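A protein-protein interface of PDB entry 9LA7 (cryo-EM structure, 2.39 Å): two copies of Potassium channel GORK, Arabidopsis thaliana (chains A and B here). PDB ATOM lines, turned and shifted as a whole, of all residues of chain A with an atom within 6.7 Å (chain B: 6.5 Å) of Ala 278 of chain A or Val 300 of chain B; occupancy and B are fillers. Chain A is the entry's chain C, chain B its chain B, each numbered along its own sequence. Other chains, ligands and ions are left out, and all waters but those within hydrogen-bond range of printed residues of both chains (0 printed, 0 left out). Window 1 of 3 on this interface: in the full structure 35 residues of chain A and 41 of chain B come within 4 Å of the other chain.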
ATOM      1  N   ALA A 273      28.904  20.234   6.841  1.00  0.00           N
ATOM      2  CA  ALA A 273      29.186  21.658   6.687  1.00  0.00           C
ATOM      3  C   ALA A 273      28.553  22.482   7.803  1.00  0.00           C
ATOM      4  O   ALA A 273      29.166  23.431   8.301  1.00  0.00           O
ATOM      5  CB  ALA A 273      28.706  22.137   5.320  1.00  0.00           C
ATOM      6  N   ILE A 274      27.324  22.149   8.197  1.00  0.00           N
ATOM      7  CA  ILE A 274      26.650  22.863   9.277  1.00  0.00           C
ATOM      8  C   ILE A 274      27.350  22.602  10.603  1.00  0.00           C
ATOM      9  O   ILE A 274      27.579  23.523  11.394  1.00  0.00           O
ATOM     10  CB  ILE A 274      25.164  22.458   9.338  1.00  0.00           C
ATOM     11  CG1 ILE A 274      24.378  23.053   8.168  1.00  0.00           C
ATOM     12  CG2 ILE A 274      24.544  22.885  10.654  1.00  0.00           C
ATOM     13  CD1 ILE A 274      23.999  24.494   8.355  1.00  0.00           C
ATOM     14  N   VAL A 275      27.699  21.340  10.865  1.00  0.00           N
ATOM     15  CA  VAL A 275      28.375  20.982  12.104  1.00  0.00           C
ATOM     16  C   VAL A 275      29.742  21.632  12.221  1.00  0.00           C
ATOM     17  O   VAL A 275      30.124  22.064  13.314  1.00  0.00           O
ATOM     18  CB  VAL A 275      28.453  19.443  12.183  1.00  0.00           C
ATOM     19  CG1 VAL A 275      29.566  18.990  13.103  1.00  0.00           C
ATOM     20  CG2 VAL A 275      27.114  18.877  12.617  1.00  0.00           C
ATOM     21  N   THR A 276      30.410  21.839  11.095  1.00  0.00           N
ATOM     22  CA  THR A 276      31.714  22.519  11.069  1.00  0.00           C
ATOM     23  C   THR A 276      31.508  24.007  11.206  1.00  0.00           C
ATOM     24  O   THR A 276      32.286  24.641  11.922  1.00  0.00           O
ATOM     25  CB  THR A 276      32.417  22.167   9.761  1.00  0.00           C
ATOM     26  OG1 THR A 276      32.612  20.760   9.833  1.00  0.00           O
ATOM     27  CG2 THR A 276      33.720  22.925   9.592  1.00  0.00           C
ATOM     28  N   MET A 277      30.475  24.549  10.571  1.00  0.00           N
ATOM     29  CA  MET A 277      30.205  25.981  10.644  1.00  0.00           C
ATOM     30  C   MET A 277      29.915  26.439  12.068  1.00  0.00           C
ATOM     31  O   MET A 277      30.301  27.548  12.454  1.00  0.00           O
ATOM     32  CB  MET A 277      29.057  26.320   9.689  1.00  0.00           C
ATOM     33  CG  MET A 277      28.427  27.688   9.856  1.00  0.00           C
ATOM     34  SD  MET A 277      26.656  27.550   9.532  1.00  0.00           S
ATOM     35  CE  MET A 277      26.003  27.166  11.152  1.00  0.00           C
ATOM     36  N   ALA A 278      29.248  25.613  12.865  1.00  0.00           N
ATOM     37  CA  ALA A 278      28.994  25.949  14.259  1.00  0.00           C
ATOM     38  C   ALA A 278      30.131  25.543  15.183  1.00  0.00           C
ATOM     39  O   ALA A 278      30.015  25.720  16.400  1.00  0.00           O
ATOM     40  CB  ALA A 278      27.697  25.306  14.739  1.00  0.00           C
ATOM     41  N   THR A 279      31.213  24.990  14.633  1.00  0.00           N
ATOM     42  CA  THR A 279      32.391  24.578  15.398  1.00  0.00           C
ATOM     43  C   THR A 279      32.052  23.478  16.399  1.00  0.00           C
ATOM     44  O   THR A 279      32.776  23.252  17.370  1.00  0.00           O
ATOM     45  CB  THR A 279      33.061  25.766  16.098  1.00  0.00           C
ATOM     46  OG1 THR A 279      32.223  26.246  17.156  1.00  0.00           O
ATOM     47  CG2 THR A 279      33.317  26.893  15.113  1.00  0.00           C
ATOM     48  N   VAL A 280      30.932  22.781  16.179  1.00  0.00           N
ATOM     49  CA  VAL A 280      30.630  21.601  17.047  1.00  0.00           C
ATOM     50  C   VAL A 280      31.704  20.560  16.709  1.00  0.00           C
ATOM     51  O   VAL A 280      32.565  20.299  17.578  1.00  0.00           O
ATOM     52  CB  VAL A 280      29.214  21.035  16.832  1.00  0.00           C
ATOM     53  CG1 VAL A 280      28.674  20.370  18.091  1.00  0.00           C
ATOM     54  CG2 VAL A 280      28.250  22.104  16.334  1.00  0.00           C
ATOM     55  N   GLY A 281      31.642  19.976  15.509  1.00  0.00           N
ATOM     56  CA  GLY A 281      32.729  19.088  15.050  1.00  0.00           C
ATOM     57  C   GLY A 281      32.670  17.654  15.534  1.00  0.00           C
ATOM     58  O   GLY A 281      33.706  17.181  16.046  1.00  0.00           O
ATOM     59  N   TYR A 282      31.592  16.923  15.319  1.00  0.00           N
ATOM     60  CA  TYR A 282      31.456  15.553  15.871  1.00  0.00           C
ATOM     61  C   TYR A 282      32.649  14.684  15.483  1.00  0.00           C
ATOM     62  O   TYR A 282      33.225  14.078  16.382  1.00  0.00           O
ATOM     63  CB  TYR A 282      30.110  14.995  15.418  1.00  0.00           C
ATOM     64  CG  TYR A 282      28.907  15.774  15.913  1.00  0.00           C
ATOM     65  CD1 TYR A 282      28.615  15.867  17.266  1.00  0.00           C
ATOM     66  CD2 TYR A 282      28.063  16.403  15.016  1.00  0.00           C
ATOM     67  CE1 TYR A 282      27.515  16.575  17.711  1.00  0.00           C
ATOM     68  CE2 TYR A 282      26.958  17.108  15.447  1.00  0.00           C
ATOM     69  CZ  TYR A 282      26.684  17.193  16.796  1.00  0.00           C
ATOM     70  OH  TYR A 282      25.587  17.897  17.175  1.00  0.00           O
ATOM     71  N   TYR A 299      37.773  26.400   4.799  1.00  0.00           N
ATOM     72  CA  TYR A 299      36.406  26.642   5.235  1.00  0.00           C
ATOM     73  C   TYR A 299      36.349  27.027   6.706  1.00  0.00           C
ATOM     74  O   TYR A 299      35.647  27.971   7.076  1.00  0.00           O
ATOM     75  CB  TYR A 299      35.549  25.406   4.968  1.00  0.00           C
ATOM     76  CG  TYR A 299      34.112  25.556   5.402  1.00  0.00           C
ATOM     77  CD1 TYR A 299      33.369  26.670   5.038  1.00  0.00           C
ATOM     78  CD2 TYR A 299      33.502  24.591   6.185  1.00  0.00           C
ATOM     79  CE1 TYR A 299      32.058  26.813   5.437  1.00  0.00           C
ATOM     80  CE2 TYR A 299      32.192  24.724   6.589  1.00  0.00           C
ATOM     81  CZ  TYR A 299      31.474  25.835   6.213  1.00  0.00           C
ATOM     82  OH  TYR A 299      30.168  25.967   6.616  1.00  0.00           O
ATOM     83  N   ASP A 303      35.202  30.532   8.239  1.00  0.00           N
ATOM     84  CA  ASP A 303      34.037  30.526   9.111  1.00  0.00           C
ATOM     85  C   ASP A 303      34.380  30.987  10.519  1.00  0.00           C
ATOM     86  O   ASP A 303      33.498  31.444  11.243  1.00  0.00           O
ATOM     87  CB  ASP A 303      33.411  29.133   9.145  1.00  0.00           C
ATOM     88  CG  ASP A 303      31.906  29.171   8.983  1.00  0.00           C
ATOM     89  OD1 ASP A 303      31.233  29.835   9.799  1.00  0.00           O
ATOM     90  OD2 ASP A 303      31.393  28.542   8.035  1.00  0.00           O
ATOM     91  N   THR B 276      26.601  19.512  22.324  1.00  0.00           N
ATOM     92  CA  THR B 276      26.411  20.249  21.082  1.00  0.00           C
ATOM     93  C   THR B 276      25.981  21.694  21.296  1.00  0.00           C
ATOM     94  O   THR B 276      26.284  22.542  20.451  1.00  0.00           O
ATOM     95  CB  THR B 276      25.386  19.545  20.185  1.00  0.00           C
ATOM     96  OG1 THR B 276      24.082  19.661  20.758  1.00  0.00           O
ATOM     97  CG2 THR B 276      25.740  18.087  20.037  1.00  0.00           C
ATOM     98  N   THR B 279      28.954  23.597  21.688  1.00  0.00           N
ATOM     99  CA  THR B 279      29.819  23.406  20.494  1.00  0.00           C
ATOM    100  C   THR B 279      31.047  22.590  20.858  1.00  0.00           C
ATOM    101  O   THR B 279      32.080  22.755  20.174  1.00  0.00           O
ATOM    102  CB  THR B 279      30.183  24.743  19.840  1.00  0.00           C
ATOM    103  OG1 THR B 279      31.267  25.281  20.591  1.00  0.00           O
ATOM    104  CG2 THR B 279      29.018  25.716  19.816  1.00  0.00           C
ATOM    105  N   PHE B 295      17.700  17.320  11.975  1.00  0.00           N
ATOM    106  CA  PHE B 295      17.428  17.904  13.281  1.00  0.00           C
ATOM    107  C   PHE B 295      18.687  18.494  13.898  1.00  0.00           C
ATOM    108  O   PHE B 295      18.634  19.554  14.529  1.00  0.00           O
ATOM    109  CB  PHE B 295      16.823  16.871  14.224  1.00  0.00           C
ATOM    110  CG  PHE B 295      16.818  17.308  15.654  1.00  0.00           C
ATOM    111  CD1 PHE B 295      15.840  18.168  16.120  1.00  0.00           C
ATOM    112  CD2 PHE B 295      17.802  16.884  16.528  1.00  0.00           C
ATOM    113  CE1 PHE B 295      15.841  18.588  17.428  1.00  0.00           C
ATOM    114  CE2 PHE B 295      17.807  17.302  17.835  1.00  0.00           C
ATOM    115  CZ  PHE B 295      16.825  18.152  18.284  1.00  0.00           C
ATOM    116  N   VAL B 296      19.824  17.808  13.758  1.00  0.00           N
ATOM    117  CA  VAL B 296      21.063  18.331  14.319  1.00  0.00           C
ATOM    118  C   VAL B 296      21.461  19.617  13.611  1.00  0.00           C
ATOM    119  O   VAL B 296      21.940  20.557  14.243  1.00  0.00           O
ATOM    120  CB  VAL B 296      22.178  17.269  14.261  1.00  0.00           C
ATOM    121  CG1 VAL B 296      23.529  17.895  14.555  1.00  0.00           C
ATOM    122  CG2 VAL B 296      21.900  16.167  15.259  1.00  0.00           C
ATOM    123  N   MET B 297      21.245  19.694  12.297  1.00  0.00           N
ATOM    124  CA  MET B 297      21.526  20.930  11.576  1.00  0.00           C
ATOM    125  C   MET B 297      20.645  22.070  12.068  1.00  0.00           C
ATOM    126  O   MET B 297      21.135  23.180  12.313  1.00  0.00           O
ATOM    127  CB  MET B 297      21.333  20.726  10.074  1.00  0.00           C
ATOM    128  CG  MET B 297      22.370  19.839   9.423  1.00  0.00           C
ATOM    129  SD  MET B 297      22.291  19.925   7.630  1.00  0.00           S
ATOM    130  CE  MET B 297      21.157  18.592   7.270  1.00  0.00           C
ATOM    131  N   ILE B 298      19.347  21.812  12.232  1.00  0.00           N
ATOM    132  CA  ILE B 298      18.436  22.853  12.700  1.00  0.00           C
ATOM    133  C   ILE B 298      18.826  23.311  14.099  1.00  0.00           C
ATOM    134  O   ILE B 298      18.969  24.513  14.366  1.00  0.00           O
ATOM    135  CB  ILE B 298      16.983  22.348  12.659  1.00  0.00           C
ATOM    136  CG1 ILE B 298      16.522  22.151  11.215  1.00  0.00           C
ATOM    137  CG2 ILE B 298      16.061  23.298  13.406  1.00  0.00           C
ATOM    138  CD1 ILE B 298      15.345  21.218  11.079  1.00  0.00           C
ATOM    139  N   TYR B 299      19.022  22.355  15.007  1.00  0.00           N
ATOM    140  CA  TYR B 299      19.363  22.678  16.384  1.00  0.00           C
ATOM    141  C   TYR B 299      20.714  23.369  16.466  1.00  0.00           C
ATOM    142  O   TYR B 299      20.892  24.299  17.252  1.00  0.00           O
ATOM    143  CB  TYR B 299      19.353  21.405  17.229  1.00  0.00           C
ATOM    144  CG  TYR B 299      19.850  21.590  18.640  1.00  0.00           C
ATOM    145  CD1 TYR B 299      19.296  22.551  19.473  1.00  0.00           C
ATOM    146  CD2 TYR B 299      20.880  20.809  19.138  1.00  0.00           C
ATOM    147  CE1 TYR B 299      19.750  22.722  20.763  1.00  0.00           C
ATOM    148  CE2 TYR B 299      21.341  20.974  20.423  1.00  0.00           C
ATOM    149  CZ  TYR B 299      20.774  21.930  21.233  1.00  0.00           C
ATOM    150  OH  TYR B 299      21.235  22.092  22.517  1.00  0.00           O
ATOM    151  N   VAL B 300      21.669  22.944  15.644  1.00  0.00           N
ATOM    152  CA  VAL B 300      23.017  23.489  15.677  1.00  0.00           C
ATOM    153  C   VAL B 300      23.044  24.914  15.134  1.00  0.00           C
ATOM    154  O   VAL B 300      23.731  25.778  15.684  1.00  0.00           O
ATOM    155  CB  VAL B 300      23.960  22.542  14.911  1.00  0.00           C
ATOM    156  CG1 VAL B 300      25.025  23.301  14.184  1.00  0.00           C
ATOM    157  CG2 VAL B 300      24.590  21.542  15.871  1.00  0.00           C
ATOM    158  N   SER B 301      22.290  25.194  14.070  1.00  0.00           N
ATOM    159  CA  SER B 301      22.215  26.563  13.564  1.00  0.00           C
ATOM    160  C   SER B 301      21.512  27.479  14.561  1.00  0.00           C
ATOM    161  O   SER B 301      21.993  28.583  14.867  1.00  0.00           O
ATOM    162  CB  SER B 301      21.494  26.581  12.216  1.00  0.00           C
ATOM    163  OG  SER B 301      21.989  25.569  11.360  1.00  0.00           O
ATOM    164  N   PHE B 302      20.370  27.028  15.090  1.00  0.00           N
ATOM    165  CA  PHE B 302      19.660  27.825  16.081  1.00  0.00           C
ATOM    166  C   PHE B 302      20.524  28.061  17.309  1.00  0.00           C
ATOM    167  O   PHE B 302      20.533  29.161  17.870  1.00  0.00           O
ATOM    168  CB  PHE B 302      18.353  27.138  16.472  1.00  0.00           C
ATOM    169  CG  PHE B 302      17.773  27.641  17.759  1.00  0.00           C
ATOM    170  CD1 PHE B 302      17.062  28.828  17.794  1.00  0.00           C
ATOM    171  CD2 PHE B 302      17.951  26.936  18.937  1.00  0.00           C
ATOM    172  CE1 PHE B 302      16.533  29.298  18.976  1.00  0.00           C
ATOM    173  CE2 PHE B 302      17.427  27.403  20.120  1.00  0.00           C
ATOM    174  CZ  PHE B 302      16.716  28.585  20.140  1.00  0.00           C
ATOM    175  N   ASP B 303      21.271  27.043  17.733  1.00  0.00           N
ATOM    176  CA  ASP B 303      22.108  27.170  18.913  1.00  0.00           C
ATOM    177  C   ASP B 303      23.343  28.012  18.641  1.00  0.00           C
ATOM    178  O   ASP B 303      23.853  28.654  19.556  1.00  0.00           O
ATOM    179  CB  ASP B 303      22.506  25.787  19.421  1.00  0.00           C
ATOM    180  CG  ASP B 303      23.096  25.834  20.804  1.00  0.00           C
ATOM    181  OD1 ASP B 303      24.306  26.109  20.909  1.00  0.00           O
ATOM    182  OD2 ASP B 303      22.355  25.609  21.783  1.00  0.00           O
ATOM    183  N   MET B 304      23.839  28.027  17.404  1.00  0.00           N
ATOM    184  CA  MET B 304      24.883  28.979  17.051  1.00  0.00           C
ATOM    185  C   MET B 304      24.391  30.405  17.225  1.00  0.00           C
ATOM    186  O   MET B 304      25.068  31.236  17.846  1.00  0.00           O
ATOM    187  CB  MET B 304      25.341  28.756  15.612  1.00  0.00           C
ATOM    188  CG  MET B 304      26.304  29.816  15.129  1.00  0.00           C
ATOM    189  SD  MET B 304      26.789  29.599  13.420  1.00  0.00           S
ATOM    190  CE  MET B 304      25.375  30.344  12.610  1.00  0.00           C
ATOM    191  N   VAL B 305      23.197  30.698  16.707  1.00  0.00           N
ATOM    192  CA  VAL B 305      22.644  32.040  16.873  1.00  0.00           C
ATOM    193  C   VAL B 305      22.403  32.346  18.349  1.00  0.00           C
ATOM    194  O   VAL B 305      22.696  33.448  18.826  1.00  0.00           O
ATOM    195  CB  VAL B 305      21.361  32.205  16.040  1.00  0.00           C
ATOM    196  CG1 VAL B 305      20.882  33.645  16.090  1.00  0.00           C
ATOM    197  CG2 VAL B 305      21.614  31.791  14.605  1.00  0.00           C
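The backbone carbonyl oxygen of Thr 279 of chain A lies close to the backbone carbonyl oxygen of Thr 279 of chain B (2.9 Å).
The backbone NH of Val 280 of chain A is in hydrogen-bond range of the backbone carbonyl oxygen of Val 275 of chain A (3.1 Å). The side-chain hydroxyl of Ser 301 of chain B sits at hydrogen-bond distance from the backbone carbonyl oxygen of Met 297 of chain B (2.7 Å).
Of the printed residues of chain B, Ala 278 of chain A touches Thr 279 and Val 300. Printed residues of chain A within 4 Å of Val 300 of chain B: Ile 274, Ala 278, Val 280 and Tyr 282. Printed residues of chain B within 4 Å of Ile 274 of chain A: Met 297 (3.7 Å), Val 300 (3.6 Å) and Ser 301 (3.8 Å). Of the printed residues of chain A, Thr 279 of chain B touches Ala 278 (3.6 Å), Thr 279 (2.9 Å) and Val 280 (3.6 Å). Of the printed residues of chain A, Ser 301 of chain B touches Ile 274. Printed residues of chain B within 4 Å of Thr 279 of chain A: Thr 279 (2.9 Å). Gly 281 of chain A touches none of the printed residues of chain B. The nearest residue of chain B that does not touch Ala 278 of chain A is Met 304 of chain B (4.3 Å). The nearest printed residue of chain A that does not touch Val 300 of chain B is Val 275 of chain A (4.6 Å). The nearest printed residue of chain B that does not touch Val 280 of chain A is Val 296 of chain B (6.6 Å).
Among the printed residues, merely in contact across the chains: Tyr 282 of chain A with Thr 276 of chain B (2.9 Å), Tyr 282 of chain A with Val 296 of chain B (3.3 Å), Ala 278 of chain A with Val 300 of chain B (3.4 Å), Met 277 of chain A with Met 304 of chain B (3.4 Å), Ala 278 of chain A with Thr 279 of chain B (3.6 Å), Ile 274 of chain A with Val 300 of chain B (3.6 Å), Val 280 of chain A with Thr 279 of chain B (3.6 Å), Ile 274 of chain A with Met 297 of chain B (3.7 Å), Val 280 of chain A with Val 300 of chain B (3.7 Å), Val 280 of chain A with Thr 276 of chain B (3.8 Å), Ile 274 of chain A with Ser 301 of chain B (3.8 Å) and Tyr 282 of chain A with Val 300 of chain B (3.998 Å).
Thr 279 of chain B touches its own counterpart, Thr 279 of chain A.
Of the 12 printed residues of chain A, 6 touch a printed residue of chain B. Hydrophobic or aromatic side chains of chain A within 4 Å of the printed part of chain B: Ile 274, Met 277, Ala 278, Val 280 and Tyr 282. Hydrophobic or aromatic side chains of chain B within 4 Å of the printed part of chain A: Val 296, Met 297, Val 300 and Met 304.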
